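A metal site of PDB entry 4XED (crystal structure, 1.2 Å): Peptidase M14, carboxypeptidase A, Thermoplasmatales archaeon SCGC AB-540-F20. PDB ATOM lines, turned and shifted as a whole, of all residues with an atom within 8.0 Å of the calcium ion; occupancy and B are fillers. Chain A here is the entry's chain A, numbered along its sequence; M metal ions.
The backbone NH of Tyr 86 lies within hydrogen-bond range of the side-chain carboxylate of Asp 82 (3.0 Å).
OD1 of Asp 82 lies within hydrogen-bond range of N of Asn 85 (3.1 Å).
The side-chain carboxylate (OD1) of Asp 82 lies close to the backbone NH (N) of Leu 84, 3.2 Å away.
The backbone NH (N) of Gly 35 sits close to the side-chain carboxylate (OD1) of Asp 32, 3.4 Å away.
Of the 20 residues printed, 6 come within 4 Å of the calcium ion.
The nearest printed residue that does not touch the calcium ion is Pro 6 (4.5 Å).
The calcium ion is bound by O of Asp 5 (2.3 Å), OD2 of Asp 36 (2.3 Å), OD2 of Asp 82 (2.4 Å), OD2 of Asp 32 (2.4 Å), OD1 of Asn 4 (2.4 Å), OD1 of Asn 34 (2.5 Å) and OD1 of Asp 32 (2.6 Å).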
ATOM      1  N   ALA A   3      -9.184  25.374  -2.746  1.00  0.00           N
ATOM      2  CA  ALA A   3     -10.493  25.012  -2.142  1.00  0.00           C
ATOM      3  C   ALA A   3     -10.316  24.103  -0.915  1.00  0.00           C
ATOM      4  O   ALA A   3     -11.076  24.171   0.049  1.00  0.00           O
ATOM      5  CB  ALA A   3     -11.375  24.322  -3.172  1.00  0.00           C
ATOM      6  N   ASN A   4      -9.275  23.262  -0.944  1.00  0.00           N
ATOM      7  CA  ASN A   4      -9.059  22.289   0.129  1.00  0.00           C
ATOM      8  C   ASN A   4      -8.634  22.965   1.408  1.00  0.00           C
ATOM      9  O   ASN A   4      -7.848  23.919   1.411  1.00  0.00           O
ATOM     10  CB  ASN A   4      -8.007  21.284  -0.294  1.00  0.00           C
ATOM     11  CG  ASN A   4      -7.800  20.227   0.727  1.00  0.00           C
ATOM     12  OD1 ASN A   4      -8.755  19.640   1.215  1.00  0.00           O
ATOM     13  ND2 ASN A   4      -6.546  19.951   1.054  1.00  0.00           N
ATOM     14  N   ASP A   5      -9.159  22.444   2.514  1.00  0.00           N
ATOM     15  CA  ASP A   5      -8.769  22.917   3.863  1.00  0.00           C
ATOM     16  C   ASP A   5      -8.039  21.804   4.596  1.00  0.00           C
ATOM     17  O   ASP A   5      -8.300  20.637   4.358  1.00  0.00           O
ATOM     18  CB  ASP A   5     -10.037  23.322   4.631  1.00  0.00           C
ATOM     19  CG  ASP A   5     -10.901  24.286   3.860  1.00  0.00           C
ATOM     20  OD1 ASP A   5     -10.430  25.423   3.624  1.00  0.00           O
ATOM     21  OD2 ASP A   5     -12.044  23.907   3.457  1.00  0.00           O
ATOM     22  N   PRO A   6      -7.144  22.173   5.532  1.00  0.00           N
ATOM     23  CA  PRO A   6      -6.446  21.135   6.301  1.00  0.00           C
ATOM     24  C   PRO A   6      -7.348  20.562   7.372  1.00  0.00           C
ATOM     25  O   PRO A   6      -8.341  21.187   7.764  1.00  0.00           O
ATOM     26  CB  PRO A   6      -5.282  21.888   6.949  1.00  0.00           C
ATOM     27  CG  PRO A   6      -5.821  23.243   7.155  1.00  0.00           C
ATOM     28  CD  PRO A   6      -6.786  23.522   6.010  1.00  0.00           C
ATOM     29  N   PRO A   7      -7.007  19.364   7.871  1.00  0.00           N
ATOM     30  CA  PRO A   7      -7.797  18.843   8.978  1.00  0.00           C
ATOM     31  C   PRO A   7      -7.728  19.765  10.171  1.00  0.00           C
ATOM     32  O   PRO A   7      -6.780  20.549  10.365  1.00  0.00           O
ATOM     33  CB  PRO A   7      -7.112  17.506   9.296  1.00  0.00           C
ATOM     34  CG  PRO A   7      -6.408  17.117   8.055  1.00  0.00           C
ATOM     35  CD  PRO A   7      -5.940  18.417   7.465  1.00  0.00           C
ATOM     36  N   ASN A   8      -8.775  19.649  10.991  1.00  0.00           N
ATOM     37  CA  ASN A   8      -8.761  20.268  12.305  1.00  0.00           C
ATOM     38  C   ASN A   8      -7.699  19.649  13.194  1.00  0.00           C
ATOM     39  O   ASN A   8      -7.199  18.544  12.950  1.00  0.00           O
ATOM     40  CB  ASN A   8     -10.159  20.185  12.880  1.00  0.00           C
ATOM     41  CG  ASN A   8     -11.112  21.036  12.100  1.00  0.00           C
ATOM     42  OD1 ASN A   8     -10.857  22.218  11.892  1.00  0.00           O
ATOM     43  ND2 ASN A   8     -12.151  20.430  11.567  1.00  0.00           N
ATOM     44  N   THR A  31     -11.569  15.783  12.553  1.00  0.00           N
ATOM     45  CA  THR A  31     -12.325  15.833  11.316  1.00  0.00           C
ATOM     46  C   THR A  31     -11.594  16.712  10.309  1.00  0.00           C
ATOM     47  O   THR A  31     -10.821  17.586  10.646  1.00  0.00           O
ATOM     48  CB  THR A  31     -13.751  16.428  11.535  1.00  0.00           C
ATOM     49  OG1 THR A  31     -13.671  17.773  11.985  1.00  0.00           O
ATOM     50  CG2 THR A  31     -14.512  15.661  12.581  1.00  0.00           C
ATOM     51  N   ASP A  32     -11.858  16.429   9.036  1.00  0.00           N
ATOM     52  CA  ASP A  32     -11.435  17.301   7.959  1.00  0.00           C
ATOM     53  C   ASP A  32     -12.655  18.084   7.465  1.00  0.00           C
ATOM     54  O   ASP A  32     -13.700  17.481   7.253  1.00  0.00           O
ATOM     55  CB  ASP A  32     -10.818  16.451   6.843  1.00  0.00           C
ATOM     56  CG  ASP A  32     -10.323  17.288   5.669  1.00  0.00           C
ATOM     57  OD1 ASP A  32     -11.163  17.624   4.781  1.00  0.00           O
ATOM     58  OD2 ASP A  32      -9.123  17.667   5.634  1.00  0.00           O
ATOM     59  N   PRO A  33     -12.515  19.403   7.225  1.00  0.00           N
ATOM     60  CA  PRO A  33     -13.675  20.225   6.856  1.00  0.00           C
ATOM     61  C   PRO A  33     -14.307  19.826   5.548  1.00  0.00           C
ATOM     62  O   PRO A  33     -15.471  20.166   5.321  1.00  0.00           O
ATOM     63  CB  PRO A  33     -13.087  21.631   6.740  1.00  0.00           C
ATOM     64  CG  PRO A  33     -11.905  21.642   7.624  1.00  0.00           C
ATOM     65  CD  PRO A  33     -11.337  20.254   7.524  1.00  0.00           C
ATOM     66  N   ASN A  34     -13.545  19.144   4.696  1.00  0.00           N
ATOM     67  CA  ASN A  34     -14.025  18.720   3.394  1.00  0.00           C
ATOM     68  C   ASN A  34     -14.489  17.275   3.405  1.00  0.00           C
ATOM     69  O   ASN A  34     -14.887  16.742   2.360  1.00  0.00           O
ATOM     70  CB  ASN A  34     -12.918  18.891   2.358  1.00  0.00           C
ATOM     71  CG  ASN A  34     -12.176  20.194   2.515  1.00  0.00           C
ATOM     72  OD1 ASN A  34     -11.019  20.239   2.917  1.00  0.00           O
ATOM     73  ND2 ASN A  34     -12.855  21.288   2.212  1.00  0.00           N
ATOM     74  N   GLY A  35     -14.416  16.645   4.587  1.00  0.00           N
ATOM     75  CA  GLY A  35     -14.770  15.249   4.747  1.00  0.00           C
ATOM     76  C   GLY A  35     -13.722  14.258   4.259  1.00  0.00           C
ATOM     77  O   GLY A  35     -14.006  13.062   4.137  1.00  0.00           O
ATOM     78  N   ASP A  36     -12.514  14.745   3.992  1.00  0.00           N
ATOM     79  CA  ASP A  36     -11.447  13.922   3.447  1.00  0.00           C
ATOM     80  C   ASP A  36     -10.984  12.879   4.463  1.00  0.00           C
ATOM     81  O   ASP A  36     -10.998  13.117   5.662  1.00  0.00           O
ATOM     82  CB  ASP A  36     -10.231  14.795   3.123  1.00  0.00           C
ATOM     83  CG  ASP A  36     -10.518  15.861   2.081  1.00  0.00           C
ATOM     84  OD1 ASP A  36     -11.379  15.646   1.195  1.00  0.00           O
ATOM     85  OD2 ASP A  36      -9.830  16.898   2.114  1.00  0.00           O
ATOM     86  N   ASN A  37     -10.560  11.726   3.955  1.00  0.00           N
ATOM     87  CA  ASN A  37      -9.808  10.777   4.750  1.00  0.00           C
ATOM     88  C   ASN A  37      -8.518  11.426   5.216  1.00  0.00           C
ATOM     89  O   ASN A  37      -7.975  12.322   4.550  1.00  0.00           O
ATOM     90  CB  ASN A  37      -9.473   9.536   3.948  1.00  0.00           C
ATOM     91  CG  ASN A  37     -10.660   8.667   3.655  1.00  0.00           C
ATOM     92  OD1 ASN A  37     -11.742   8.791   4.253  1.00  0.00           O
ATOM     93  ND2 ASN A  37     -10.479   7.768   2.724  1.00  0.00           N
ATOM     94  N   ILE A  38      -8.039  11.003   6.379  1.00  0.00           N
ATOM     95  CA  ILE A  38      -6.800  11.558   6.940  1.00  0.00           C
ATOM     96  C   ILE A  38      -5.880  10.492   7.541  1.00  0.00           C
ATOM     97  O   ILE A  38      -6.320   9.398   7.901  1.00  0.00           O
ATOM     98  CB  ILE A  38      -7.027  12.698   8.017  1.00  0.00           C
ATOM     99  CG1 ILE A  38      -7.481  12.150   9.397  1.00  0.00           C
ATOM    100  CG2 ILE A  38      -7.983  13.750   7.491  1.00  0.00           C
ATOM    101  CD1 ILE A  38      -8.877  11.616   9.451  1.00  0.00           C
ATOM    102  N   LYS A  81      -3.095  14.838   8.441  1.00  0.00           N
ATOM    103  CA  LYS A  81      -3.049  15.427   7.116  1.00  0.00           C
ATOM    104  C   LYS A  81      -4.044  14.709   6.244  1.00  0.00           C
ATOM    105  O   LYS A  81      -4.316  13.529   6.400  1.00  0.00           O
ATOM    106  CB  LYS A  81      -1.657  15.385   6.510  1.00  0.00           C
ATOM    107  CG  LYS A  81      -1.229  14.033   6.009  1.00  0.00           C
ATOM    108  CD  LYS A  81       0.211  14.081   5.489  1.00  0.00           C
ATOM    109  CE  LYS A  81       0.670  12.706   5.123  1.00  0.00           C
ATOM    110  NZ  LYS A  81       2.037  12.715   4.530  1.00  0.00           N
ATOM    111  N   ASP A  82      -4.634  15.456   5.337  1.00  0.00           N
ATOM    112  CA  ASP A  82      -5.573  14.840   4.434  1.00  0.00           C
ATOM    113  C   ASP A  82      -4.881  14.187   3.224  1.00  0.00           C
ATOM    114  O   ASP A  82      -3.680  14.116   3.178  1.00  0.00           O
ATOM    115  CB  ASP A  82      -6.657  15.857   4.025  1.00  0.00           C
ATOM    116  CG  ASP A  82      -6.129  17.064   3.261  1.00  0.00           C
ATOM    117  OD1 ASP A  82      -5.006  17.063   2.732  1.00  0.00           O
ATOM    118  OD2 ASP A  82      -6.919  18.036   3.149  1.00  0.00           O
ATOM    119  N   ILE A  83      -5.667  13.708   2.259  1.00  0.00           N
ATOM    120  CA  ILE A  83      -5.145  12.970   1.133  1.00  0.00           C
ATOM    121  C   ILE A  83      -4.284  13.855   0.250  1.00  0.00           C
ATOM    122  O   ILE A  83      -3.360  13.369  -0.395  1.00  0.00           O
ATOM    123  CB  ILE A  83      -6.302  12.337   0.310  1.00  0.00           C
ATOM    124  CG1 ILE A  83      -7.113  11.411   1.211  1.00  0.00           C
ATOM    125  CG2 ILE A  83      -5.780  11.598  -0.914  1.00  0.00           C
ATOM    126  CD1 ILE A  83      -6.269  10.400   2.051  1.00  0.00           C
ATOM    127  N   LEU A  84      -4.582  15.161   0.227  1.00  0.00           N
ATOM    128  CA  LEU A  84      -3.751  16.159  -0.453  1.00  0.00           C
ATOM    129  C   LEU A  84      -2.559  16.645   0.366  1.00  0.00           C
ATOM    130  O   LEU A  84      -1.844  17.563  -0.048  1.00  0.00           O
ATOM    131  CB  LEU A  84      -4.638  17.336  -0.869  1.00  0.00           C
ATOM    132  CG  LEU A  84      -5.640  17.016  -2.003  1.00  0.00           C
ATOM    133  CD1 LEU A  84      -6.702  18.079  -2.100  1.00  0.00           C
ATOM    134  CD2 LEU A  84      -4.974  16.810  -3.371  1.00  0.00           C
ATOM    135  N   ASN A  85      -2.320  16.012   1.502  1.00  0.00           N
ATOM    136  CA  ASN A  85      -1.138  16.271   2.325  1.00  0.00           C
ATOM    137  C   ASN A  85      -1.105  17.632   3.012  1.00  0.00           C
ATOM    138  O   ASN A  85      -0.038  18.073   3.450  1.00  0.00           O
ATOM    139  CB  ASN A  85       0.147  15.941   1.561  1.00  0.00           C
ATOM    140  CG  ASN A  85       0.183  14.486   1.186  1.00  0.00           C
ATOM    141  OD1 ASN A  85       0.056  13.622   2.042  1.00  0.00           O
ATOM    142  ND2 ASN A  85       0.334  14.206  -0.104  1.00  0.00           N
ATOM    143  N   TYR A  86      -2.284  18.228   3.178  1.00  0.00           N
ATOM    144  CA  TYR A  86      -2.429  19.477   3.898  1.00  0.00           C
ATOM    145  C   TYR A  86      -2.476  19.114   5.393  1.00  0.00           C
ATOM    146  O   TYR A  86      -3.345  18.361   5.828  1.00  0.00           O
ATOM    147  CB  TYR A  86      -3.705  20.162   3.448  1.00  0.00           C
ATOM    148  CG  TYR A  86      -3.749  21.673   3.520  1.00  0.00           C
ATOM    149  CD1 TYR A  86      -2.692  22.430   4.008  1.00  0.00           C
ATOM    150  CD2 TYR A  86      -4.881  22.353   3.086  1.00  0.00           C
ATOM    151  CE1 TYR A  86      -2.771  23.836   4.035  1.00  0.00           C
ATOM    152  CE2 TYR A  86      -4.964  23.751   3.116  1.00  0.00           C
ATOM    153  CZ  TYR A  86      -3.914  24.477   3.608  1.00  0.00           C
ATOM    154  OH  TYR A  86      -3.988  25.860   3.643  1.00  0.00           O
HETATM  155 CA    CA M   1      -9.173  18.706   3.435  1.00  0.00          CA
